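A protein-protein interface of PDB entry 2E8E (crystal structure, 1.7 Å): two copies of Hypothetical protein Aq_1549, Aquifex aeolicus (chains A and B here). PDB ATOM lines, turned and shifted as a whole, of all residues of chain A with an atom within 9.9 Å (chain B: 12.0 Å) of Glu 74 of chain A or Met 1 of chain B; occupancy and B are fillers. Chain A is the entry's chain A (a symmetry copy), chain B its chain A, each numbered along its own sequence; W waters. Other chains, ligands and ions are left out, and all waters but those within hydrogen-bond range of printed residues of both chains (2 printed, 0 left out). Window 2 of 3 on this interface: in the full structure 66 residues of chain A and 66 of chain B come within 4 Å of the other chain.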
ATOM      1  N   LYS A  69      10.717  20.998  -2.755  1.00  0.00           N
ATOM      2  CA  LYS A  69       9.789  19.882  -2.715  1.00  0.00           C
ATOM      3  C   LYS A  69       8.465  20.346  -3.293  1.00  0.00           C
ATOM      4  O   LYS A  69       7.882  21.325  -2.823  1.00  0.00           O
ATOM      5  CB  LYS A  69       9.573  19.396  -1.281  1.00  0.00           C
ATOM      6  CG  LYS A  69       8.511  18.311  -1.170  1.00  0.00           C
ATOM      7  CD  LYS A  69       8.329  17.829   0.261  1.00  0.00           C
ATOM      8  CE  LYS A  69       9.613  17.242   0.817  1.00  0.00           C
ATOM      9  NZ  LYS A  69       9.422  16.662   2.179  1.00  0.00           N
ATOM     10  N   GLY A  70       7.991  19.644  -4.315  1.00  0.00           N
ATOM     11  CA  GLY A  70       6.733  20.023  -4.924  1.00  0.00           C
ATOM     12  C   GLY A  70       5.703  18.921  -4.799  1.00  0.00           C
ATOM     13  O   GLY A  70       6.023  17.750  -4.986  1.00  0.00           O
ATOM     14  N   LYS A  71       4.473  19.298  -4.465  1.00  0.00           N
ATOM     15  CA  LYS A  71       3.372  18.345  -4.329  1.00  0.00           C
ATOM     16  C   LYS A  71       2.396  18.610  -5.468  1.00  0.00           C
ATOM     17  O   LYS A  71       1.873  19.719  -5.604  1.00  0.00           O
ATOM     18  CB  LYS A  71       2.679  18.523  -2.977  1.00  0.00           C
ATOM     19  CG  LYS A  71       3.553  18.152  -1.795  1.00  0.00           C
ATOM     20  CD  LYS A  71       2.834  18.395  -0.475  1.00  0.00           C
ATOM     21  CE  LYS A  71       3.676  17.933   0.707  1.00  0.00           C
ATOM     22  NZ  LYS A  71       4.996  18.622   0.762  1.00  0.00           N
ATOM     23  N   ARG A  72       2.143  17.585  -6.276  1.00  0.00           N
ATOM     24  CA  ARG A  72       1.277  17.723  -7.442  1.00  0.00           C
ATOM     25  C   ARG A  72      -0.186  17.353  -7.258  1.00  0.00           C
ATOM     26  O   ARG A  72      -0.525  16.464  -6.476  1.00  0.00           O
ATOM     27  CB  ARG A  72       1.835  16.883  -8.593  1.00  0.00           C
ATOM     28  CG  ARG A  72       3.298  17.138  -8.889  1.00  0.00           C
ATOM     29  CD  ARG A  72       3.814  16.190  -9.952  1.00  0.00           C
ATOM     30  NE  ARG A  72       3.195  16.420 -11.252  1.00  0.00           N
ATOM     31  CZ  ARG A  72       3.545  15.775 -12.359  1.00  0.00           C
ATOM     32  NH1 ARG A  72       4.500  14.855 -12.312  1.00  0.00           N
ATOM     33  NH2 ARG A  72       2.973  16.075 -13.513  1.00  0.00           N
ATOM     34  N   ARG A  73      -1.041  18.046  -8.004  1.00  0.00           N
ATOM     35  CA  ARG A  73      -2.473  17.791  -7.995  1.00  0.00           C
ATOM     36  C   ARG A  73      -2.657  16.401  -8.590  1.00  0.00           C
ATOM     37  O   ARG A  73      -1.810  15.930  -9.349  1.00  0.00           O
ATOM     38  CB  ARG A  73      -3.200  18.832  -8.854  1.00  0.00           C
ATOM     39  CG  ARG A  73      -4.693  18.600  -8.990  1.00  0.00           C
ATOM     40  CD  ARG A  73      -5.397  19.797  -9.603  1.00  0.00           C
ATOM     41  NE  ARG A  73      -4.953  20.084 -10.964  1.00  0.00           N
ATOM     42  CZ  ARG A  73      -5.400  21.105 -11.688  1.00  0.00           C
ATOM     43  NH1 ARG A  73      -6.302  21.934 -11.178  1.00  0.00           N
ATOM     44  NH2 ARG A  73      -4.949  21.301 -12.918  1.00  0.00           N
ATOM     45  N   GLU A  74      -3.765  15.745  -8.266  1.00  0.00           N
ATOM     46  CA  GLU A  74      -4.002  14.398  -8.766  1.00  0.00           C
ATOM     47  C   GLU A  74      -4.712  14.312 -10.115  1.00  0.00           C
ATOM     48  O   GLU A  74      -4.718  13.255 -10.742  1.00  0.00           O
ATOM     49  CB  GLU A  74      -4.749  13.594  -7.694  1.00  0.00           C
ATOM     50  CG  GLU A  74      -3.890  13.405  -6.453  1.00  0.00           C
ATOM     51  CD  GLU A  74      -4.647  12.855  -5.260  1.00  0.00           C
ATOM     52  OE1 GLU A  74      -4.015  12.695  -4.194  1.00  0.00           O
ATOM     53  OE2 GLU A  74      -5.862  12.590  -5.383  1.00  0.00           O
ATOM     54  N   LYS A  75      -5.291  15.419 -10.565  1.00  0.00           N
ATOM     55  CA  LYS A  75      -5.976  15.453 -11.853  1.00  0.00           C
ATOM     56  C   LYS A  75      -5.216  16.350 -12.828  1.00  0.00           C
ATOM     57  O   LYS A  75      -4.500  17.259 -12.412  1.00  0.00           O
ATOM     58  CB  LYS A  75      -7.409  15.956 -11.669  1.00  0.00           C
ATOM     59  CG  LYS A  75      -8.256  15.016 -10.831  1.00  0.00           C
ATOM     60  CD  LYS A  75      -9.627  15.588 -10.535  1.00  0.00           C
ATOM     61  CE  LYS A  75     -10.472  14.569  -9.787  1.00  0.00           C
ATOM     62  NZ  LYS A  75      -9.794  14.102  -8.542  1.00  0.00           N
ATOM     63  N   HIS A  76      -5.375  16.089 -14.122  1.00  0.00           N
ATOM     64  CA  HIS A  76      -4.686  16.863 -15.151  1.00  0.00           C
ATOM     65  C   HIS A  76      -5.242  18.272 -15.349  1.00  0.00           C
ATOM     66  O   HIS A  76      -6.457  18.475 -15.349  1.00  0.00           O
ATOM     67  CB  HIS A  76      -4.730  16.119 -16.491  1.00  0.00           C
ATOM     68  CG  HIS A  76      -4.059  14.782 -16.465  1.00  0.00           C
ATOM     69  ND1 HIS A  76      -4.760  13.596 -16.407  1.00  0.00           N
ATOM     70  CD2 HIS A  76      -2.749  14.441 -16.498  1.00  0.00           C
ATOM     71  CE1 HIS A  76      -3.911  12.583 -16.407  1.00  0.00           C
ATOM     72  NE2 HIS A  76      -2.684  13.070 -16.462  1.00  0.00           N
ATOM     73  N   PRO A  77      -4.351  19.272 -15.501  1.00  0.00           N
ATOM     74  CA  PRO A  77      -2.891  19.109 -15.483  1.00  0.00           C
ATOM     75  C   PRO A  77      -2.383  18.963 -14.046  1.00  0.00           C
ATOM     76  O   PRO A  77      -2.833  19.668 -13.144  1.00  0.00           O
ATOM     77  CB  PRO A  77      -2.395  20.383 -16.165  1.00  0.00           C
ATOM     78  CG  PRO A  77      -3.420  21.392 -15.775  1.00  0.00           C
ATOM     79  CD  PRO A  77      -4.718  20.626 -15.954  1.00  0.00           C
ATOM     80  N   LYS A  78      -1.440  18.049 -13.847  1.00  0.00           N
ATOM     81  CA  LYS A  78      -0.904  17.778 -12.522  1.00  0.00           C
ATOM     82  C   LYS A  78       0.162  18.772 -12.078  1.00  0.00           C
ATOM     83  O   LYS A  78       1.310  18.411 -11.824  1.00  0.00           O
ATOM     84  CB  LYS A  78      -0.367  16.348 -12.477  1.00  0.00           C
ATOM     85  CG  LYS A  78      -1.449  15.313 -12.792  1.00  0.00           C
ATOM     86  CD  LYS A  78      -0.952  13.893 -12.608  1.00  0.00           C
ATOM     87  CE  LYS A  78      -2.095  12.904 -12.784  1.00  0.00           C
ATOM     88  NZ  LYS A  78      -1.665  11.496 -12.565  1.00  0.00           N
ATOM     89  N   ILE A  79      -0.243  20.033 -11.983  1.00  0.00           N
ATOM     90  CA  ILE A  79       0.651  21.105 -11.568  1.00  0.00           C
ATOM     91  C   ILE A  79       1.011  20.951 -10.093  1.00  0.00           C
ATOM     92  O   ILE A  79       0.387  20.179  -9.367  1.00  0.00           O
ATOM     93  CB  ILE A  79      -0.028  22.481 -11.727  1.00  0.00           C
ATOM     94  CG1 ILE A  79      -1.285  22.539 -10.851  1.00  0.00           C
ATOM     95  CG2 ILE A  79      -0.382  22.733 -13.190  1.00  0.00           C
ATOM     96  CD1 ILE A  79      -1.978  23.883 -10.842  1.00  0.00           C
ATOM     97  N   TYR A  80       2.025  21.687  -9.652  1.00  0.00           N
ATOM     98  CA  TYR A  80       2.401  21.664  -8.243  1.00  0.00           C
ATOM     99  C   TYR A  80       1.402  22.539  -7.493  1.00  0.00           C
ATOM    100  O   TYR A  80       1.296  23.735  -7.767  1.00  0.00           O
ATOM    101  CB  TYR A  80       3.798  22.254  -8.034  1.00  0.00           C
ATOM    102  CG  TYR A  80       4.934  21.393  -8.527  1.00  0.00           C
ATOM    103  CD1 TYR A  80       5.086  20.080  -8.082  1.00  0.00           C
ATOM    104  CD2 TYR A  80       5.880  21.906  -9.413  1.00  0.00           C
ATOM    105  CE1 TYR A  80       6.159  19.300  -8.503  1.00  0.00           C
ATOM    106  CE2 TYR A  80       6.954  21.137  -9.844  1.00  0.00           C
ATOM    107  CZ  TYR A  80       7.088  19.836  -9.383  1.00  0.00           C
ATOM    108  OH  TYR A  80       8.159  19.085  -9.795  1.00  0.00           O
ATOM    109  N   GLU A  81       0.663  21.958  -6.555  1.00  0.00           N
ATOM    110  CA  GLU A  81      -0.290  22.744  -5.785  1.00  0.00           C
ATOM    111  C   GLU A  81       0.481  23.452  -4.680  1.00  0.00           C
ATOM    112  O   GLU A  81       0.031  24.458  -4.125  1.00  0.00           O
ATOM    113  CB  GLU A  81      -1.366  21.847  -5.168  1.00  0.00           C
ATOM    114  CG  GLU A  81      -2.116  21.000  -6.182  1.00  0.00           C
ATOM    115  CD  GLU A  81      -3.593  20.866  -5.861  1.00  0.00           C
ATOM    116  OE1 GLU A  81      -3.931  20.506  -4.714  1.00  0.00           O
ATOM    117  OE2 GLU A  81      -4.419  21.118  -6.763  1.00  0.00           O
ATOM    118  N   GLU A  82       1.657  22.920  -4.378  1.00  0.00           N
ATOM    119  CA  GLU A  82       2.503  23.478  -3.337  1.00  0.00           C
ATOM    120  C   GLU A  82       3.967  23.258  -3.677  1.00  0.00           C
ATOM    121  O   GLU A  82       4.341  22.213  -4.202  1.00  0.00           O
ATOM    122  CB  GLU A  82       2.178  22.810  -1.995  1.00  0.00           C
ATOM    123  CG  GLU A  82       3.205  23.043  -0.901  1.00  0.00           C
ATOM    124  CD  GLU A  82       2.905  22.252   0.363  1.00  0.00           C
ATOM    125  OE1 GLU A  82       3.862  21.744   0.981  1.00  0.00           O
ATOM    126  OE2 GLU A  82       1.719  22.145   0.743  1.00  0.00           O
ATOM    127  N   ILE A  83       4.788  24.264  -3.401  1.00  0.00           N
ATOM    128  CA  ILE A  83       6.222  24.158  -3.633  1.00  0.00           C
ATOM    129  C   ILE A  83       6.910  24.696  -2.392  1.00  0.00           C
ATOM    130  O   ILE A  83       6.701  25.849  -2.015  1.00  0.00           O
ATOM    131  CB  ILE A  83       6.699  24.997  -4.840  1.00  0.00           C
ATOM    132  CG1 ILE A  83       6.027  24.509  -6.125  1.00  0.00           C
ATOM    133  CG2 ILE A  83       8.225  24.884  -4.966  1.00  0.00           C
ATOM    134  CD1 ILE A  83       6.473  25.249  -7.366  1.00  0.00           C
ATOM    135  N   THR A 120       0.481  28.446  -7.687  1.00  0.00           N
ATOM    136  CA  THR A 120       0.819  27.512  -6.612  1.00  0.00           C
ATOM    137  C   THR A 120       0.998  28.166  -5.238  1.00  0.00           C
ATOM    138  O   THR A 120       1.143  29.387  -5.132  1.00  0.00           O
ATOM    139  CB  THR A 120       2.121  26.750  -6.962  1.00  0.00           C
ATOM    140  OG1 THR A 120       2.300  25.654  -6.061  1.00  0.00           O
ATOM    141  CG2 THR A 120       3.324  27.678  -6.854  1.00  0.00           C
ATOM    142  N   ASN A 121       0.978  27.351  -4.186  1.00  0.00           N
ATOM    143  CA  ASN A 121       1.179  27.850  -2.831  1.00  0.00           C
ATOM    144  C   ASN A 121       2.659  27.695  -2.523  1.00  0.00           C
ATOM    145  O   ASN A 121       3.179  26.578  -2.464  1.00  0.00           O
ATOM    146  CB  ASN A 121       0.351  27.057  -1.812  1.00  0.00           C
ATOM    147  CG  ASN A 121       0.680  27.438  -0.372  1.00  0.00           C
ATOM    148  OD1 ASN A 121       1.073  28.572  -0.091  1.00  0.00           O
ATOM    149  ND2 ASN A 121       0.503  26.497   0.547  1.00  0.00           N
ATOM    150  N   MET B   1      -1.264  12.704  -4.163  1.00  0.00           N
ATOM    151  CA  MET B   1      -0.460  13.853  -4.665  1.00  0.00           C
ATOM    152  C   MET B   1       0.996  13.427  -4.794  1.00  0.00           C
ATOM    153  O   MET B   1       1.654  13.145  -3.794  1.00  0.00           O
ATOM    154  CB  MET B   1      -0.568  15.036  -3.697  1.00  0.00           C
ATOM    155  CG  MET B   1      -1.957  15.651  -3.605  1.00  0.00           C
ATOM    156  SD  MET B   1      -2.023  17.079  -2.496  1.00  0.00           S
ATOM    157  CE  MET B   1      -1.598  18.396  -3.612  1.00  0.00           C
ATOM    158  N   GLU B   2       1.499  13.373  -6.022  1.00  0.00           N
ATOM    159  CA  GLU B   2       2.885  12.971  -6.220  1.00  0.00           C
ATOM    160  C   GLU B   2       3.830  14.043  -5.710  1.00  0.00           C
ATOM    161  O   GLU B   2       3.578  15.241  -5.861  1.00  0.00           O
ATOM    162  CB  GLU B   2       3.188  12.693  -7.695  1.00  0.00           C
ATOM    163  CG  GLU B   2       4.671  12.438  -7.945  1.00  0.00           C
ATOM    164  CD  GLU B   2       5.000  12.133  -9.395  1.00  0.00           C
ATOM    165  OE1 GLU B   2       4.370  12.734 -10.287  1.00  0.00           O
ATOM    166  OE2 GLU B   2       5.906  11.304  -9.636  1.00  0.00           O
ATOM    167  N   VAL B   3       4.922  13.598  -5.103  1.00  0.00           N
ATOM    168  CA  VAL B   3       5.922  14.499  -4.569  1.00  0.00           C
ATOM    169  C   VAL B   3       7.201  14.413  -5.392  1.00  0.00           C
ATOM    170  O   VAL B   3       7.699  13.318  -5.669  1.00  0.00           O
ATOM    171  CB  VAL B   3       6.260  14.141  -3.104  1.00  0.00           C
ATOM    172  CG1 VAL B   3       7.343  15.072  -2.573  1.00  0.00           C
ATOM    173  CG2 VAL B   3       5.011  14.227  -2.247  1.00  0.00           C
ATOM    174  N   LYS B   4       7.713  15.572  -5.800  1.00  0.00           N
ATOM    175  CA  LYS B   4       8.960  15.651  -6.553  1.00  0.00           C
ATOM    176  C   LYS B   4       9.911  16.438  -5.663  1.00  0.00           C
ATOM    177  O   LYS B   4       9.504  17.411  -5.024  1.00  0.00           O
ATOM    178  CB  LYS B   4       8.785  16.419  -7.868  1.00  0.00           C
ATOM    179  CG  LYS B   4       7.879  15.775  -8.904  1.00  0.00           C
ATOM    180  CD  LYS B   4       8.448  14.474  -9.437  1.00  0.00           C
ATOM    181  CE  LYS B   4       7.710  14.051 -10.700  1.00  0.00           C
ATOM    182  NZ  LYS B   4       8.007  12.649 -11.086  1.00  0.00           N
ATOM    183  N   GLU B   5      11.171  16.022  -5.625  1.00  0.00           N
ATOM    184  CA  GLU B   5      12.171  16.700  -4.819  1.00  0.00           C
ATOM    185  C   GLU B   5      13.492  16.840  -5.560  1.00  0.00           C
ATOM    186  O   GLU B   5      13.908  15.948  -6.293  1.00  0.00           O
ATOM    187  CB  GLU B   5      12.420  15.936  -3.511  1.00  0.00           C
ATOM    188  CG  GLU B   5      11.333  16.086  -2.464  1.00  0.00           C
ATOM    189  CD  GLU B   5      11.607  15.256  -1.221  1.00  0.00           C
ATOM    190  OE1 GLU B   5      12.778  15.197  -0.791  1.00  0.00           O
ATOM    191  OE2 GLU B   5      10.651  14.671  -0.669  1.00  0.00           O
ATOM    192  N   LYS B 108      -4.557  20.544 -21.561  1.00  0.00           N
ATOM    193  CA  LYS B 108      -4.946  19.629 -20.493  1.00  0.00           C
ATOM    194  C   LYS B 108      -3.856  18.844 -19.768  1.00  0.00           C
ATOM    195  O   LYS B 108      -3.874  18.747 -18.543  1.00  0.00           O
ATOM    196  CB  LYS B 108      -5.986  18.634 -21.021  1.00  0.00           C
ATOM    197  CG  LYS B 108      -6.372  17.553 -20.024  1.00  0.00           C
ATOM    198  CD  LYS B 108      -7.511  16.683 -20.538  1.00  0.00           C
ATOM    199  CE  LYS B 108      -7.938  15.666 -19.490  1.00  0.00           C
ATOM    200  NZ  LYS B 108      -9.102  14.848 -19.941  1.00  0.00           N
ATOM    201  N   TYR B 109      -2.911  18.286 -20.513  1.00  0.00           N
ATOM    202  CA  TYR B 109      -1.878  17.458 -19.905  1.00  0.00           C
ATOM    203  C   TYR B 109      -0.566  18.079 -19.438  1.00  0.00           C
ATOM    204  O   TYR B 109      -0.005  17.641 -18.437  1.00  0.00           O
ATOM    205  CB  TYR B 109      -1.552  16.301 -20.846  1.00  0.00           C
ATOM    206  CG  TYR B 109      -2.711  15.352 -21.047  1.00  0.00           C
ATOM    207  CD1 TYR B 109      -3.136  14.518 -20.017  1.00  0.00           C
ATOM    208  CD2 TYR B 109      -3.395  15.303 -22.261  1.00  0.00           C
ATOM    209  CE1 TYR B 109      -4.216  13.655 -20.190  1.00  0.00           C
ATOM    210  CE2 TYR B 109      -4.475  14.446 -22.443  1.00  0.00           C
ATOM    211  CZ  TYR B 109      -4.878  13.627 -21.404  1.00  0.00           C
ATOM    212  OH  TYR B 109      -5.945  12.778 -21.577  1.00  0.00           O
ATOM    213  N   CYS B 110      -0.072  19.085 -20.148  1.00  0.00           N
ATOM    214  CA  CYS B 110       1.215  19.672 -19.785  1.00  0.00           C
ATOM    215  C   CYS B 110       1.220  20.421 -18.458  1.00  0.00           C
ATOM    216  O   CYS B 110       0.735  21.552 -18.367  1.00  0.00           O
ATOM    217  CB  CYS B 110       1.703  20.595 -20.895  1.00  0.00           C
ATOM    218  SG  CYS B 110       3.442  21.052 -20.686  1.00  0.00           S
ATOM    219  N   SER B 111       1.800  19.791 -17.439  1.00  0.00           N
ATOM    220  CA  SER B 111       1.859  20.379 -16.105  1.00  0.00           C
ATOM    221  C   SER B 111       2.723  21.635 -16.016  1.00  0.00           C
ATOM    222  O   SER B 111       2.309  22.634 -15.426  1.00  0.00           O
ATOM    223  CB  SER B 111       2.368  19.344 -15.094  1.00  0.00           C
ATOM    224  OG  SER B 111       1.477  18.243 -14.998  1.00  0.00           O
ATOM    225  N   ALA B 114       1.077  24.618 -17.807  1.00  0.00           N
ATOM    226  CA  ALA B 114      -0.106  25.080 -17.089  1.00  0.00           C
ATOM    227  C   ALA B 114       0.258  26.047 -15.967  1.00  0.00           C
ATOM    228  O   ALA B 114      -0.511  26.953 -15.645  1.00  0.00           O
ATOM    229  CB  ALA B 114      -0.861  23.892 -16.509  1.00  0.00           C
ATOM    230  N   MET B 115       1.433  25.855 -15.382  1.00  0.00           N
ATOM    231  CA  MET B 115       1.872  26.707 -14.282  1.00  0.00           C
ATOM    232  C   MET B 115       2.332  28.107 -14.676  1.00  0.00           C
ATOM    233  O   MET B 115       2.228  29.038 -13.878  1.00  0.00           O
ATOM    234  CB  MET B 115       2.978  26.009 -13.485  1.00  0.00           C
ATOM    235  CG  MET B 115       2.475  24.819 -12.672  1.00  0.00           C
ATOM    236  SD  MET B 115       3.691  24.158 -11.513  1.00  0.00           S
ATOM    237  CE  MET B 115       3.623  25.365 -10.258  1.00  0.00           C
HETATM  238  O   HOH W   1      -0.724  16.354 -16.043  1.00  0.00           O
HETATM  239  O   HOH W   2      -0.105  13.750  -8.499  1.00  0.00           O
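Glu 74 of chain A touches just one residue of chain B: Met 1. Of the printed residues of chain A, Met 1 of chain B touches Arg 72, Glu 74 and Glu 81. Lys 71 of chain A touches just one residue of chain B: Glu 2 (3.5 Å). No residue of chain B comes within 4 Å of Arg 73 of chain A. No residue of chain B comes within 4 Å of Lys 75 of chain A. His 76 of chain A touches just these residues of chain B: Lys 108 (3.4 Å) and Tyr 109 (3.5 Å). Glu 82 of chain A touches none of the printed residues of chain B. Of the printed residues of chain A, Lys 4 of chain B touches Lys 69 (3.4 Å), Gly 70 (2.8 Å), Arg 72 (3.7 Å) and Tyr 80 (3.3 Å). Of the printed residues of chain A, Ala 114 of chain B touches Pro 77 (3.7 Å) and Ile 79 (3.5 Å). Ile 83 of chain A touches none of the printed residues of chain B. Asn 121 of chain A touches none of the printed residues of chain B. The nearest residue of chain B that does not touch Glu 74 of chain A is Glu 2 of chain B (5.4 Å). The nearest residue of chain A that does not touch Met 1 of chain B is Lys 71 of chain A (4.2 Å).
Water W1 lies within hydrogen-bond range of O of Tyr 109 of chain B, N of Lys 78 of chain A and OG of Ser 111 of chain B. Water W2 lies within hydrogen-bond range of the backbone carbonyl oxygen (O) of Arg 73 of chain A (2.9 Å), the backbone NH (N) of Glu 2 of chain B (3.0 Å) and the backbone carbonyl oxygen (O) of Arg 72 of chain A (3.4 Å).
The backbone NH (N) of Glu 81 of chain A is in hydrogen-bond range of the backbone carbonyl oxygen (O) of Lys 71 of chain A (2.7 Å). NZ of Lys 71 of chain A lies within salt-bridge range of OE1 of Glu 82 of chain A. The guanidinium group (NH2) of Arg 73 of chain A is in hydrogen-bond range of the backbone carbonyl oxygen (O) of Pro 77 of chain A (2.7 Å). The backbone carbonyl oxygen of Glu 81 of chain A sits close to the side-chain hydroxyl of Thr 120 of chain A (3.2 Å). The backbone carbonyl oxygen (O) of Glu 81 of chain A lies within hydrogen-bond range of the backbone NH (N) of Asn 121 of chain A (3.0 Å). The backbone NH (N) of Glu 82 of chain A lies within hydrogen-bond range of the side-chain hydroxyl (OG1) of Thr 120 of chain A, at 3.3 Å.
Among the printed residues, merely in contact across the chains: Lys 69 of chain A with Val 3 of chain B, Lys 69 of chain A with Lys 4 of chain B, Gly 70 of chain A with Glu 2 of chain B, Gly 70 of chain A with Val 3 of chain B, Lys 71 of chain A with Glu 2 of chain B, Arg 72 of chain A with Met 1 of chain B, Arg 72 of chain A with Lys 4 of chain B, His 76 of chain A with Lys 108 of chain B, His 76 of chain A with Tyr 109 of chain B, Pro 77 of chain A with Ala 114 of chain B, Ile 79 of chain A with Ser 111 of chain B, Ile 79 of chain A with Ala 114 of chain B, Ile 79 of chain A with Met 115 of chain B, Tyr 80 of chain A with Lys 4 of chain B, Glu 81 of chain A with Met 1 of chain B and Thr 120 of chain A with Met 115 of chain B.
The backbone NH (N) of Met 1 of chain B is in hydrogen-bond range of the side-chain carboxylate (OE1) of Glu 74 of chain A, 2.8 Å away. OE1 of Glu 2 of chain B lies within salt-bridge range of NH1 of Arg 72 of chain A (2.9 Å). O of Lys 4 of chain B sits at hydrogen-bond distance from N of Gly 70 of chain A. OE2 of Glu 5 of chain B is in salt-bridge range of NZ of Lys 69 of chain A, 3.7 Å away. The guanidinium group (NH2) of Arg 72 of chain A sits at hydrogen-bond distance from the side-chain hydroxyl (OG) of Ser 111 of chain B (3.0 Å). OG of Ser 111 of chain B lies within hydrogen-bond range of N of Lys 78 of chain A (3.1 Å). The backbone NH (N) of Tyr 80 of chain A lies within hydrogen-bond range of the side-chain sulfur (SD) of Met 115 of chain B (3.5 Å). O of Lys 108 of chain B lies close to N of Pro 77 of chain A.
Hydrophobic or aromatic side chains of chain B that line the printed part of chain A: Met 1, Val 3, Tyr 109, Ala 114 and Met 115. Printed residues of chain A that touch a printed residue of chain B: Lys 69, Gly 70, Lys 71, Arg 72, Glu 74, His 76, Pro 77, Lys 78, Ile 79, Tyr 80, Glu 81 and Thr 120. Hydrophobic or aromatic side chains of chain A that line the printed part of chain B: His 76, Pro 77, Ile 79 and Tyr 80. Among the printed residues, 24 pairs touch across the chains.
No position is printed for both chains. Of the 24 pairs that touch across the chains among the printed residues, none has its exchanged pair printed and touching as well.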
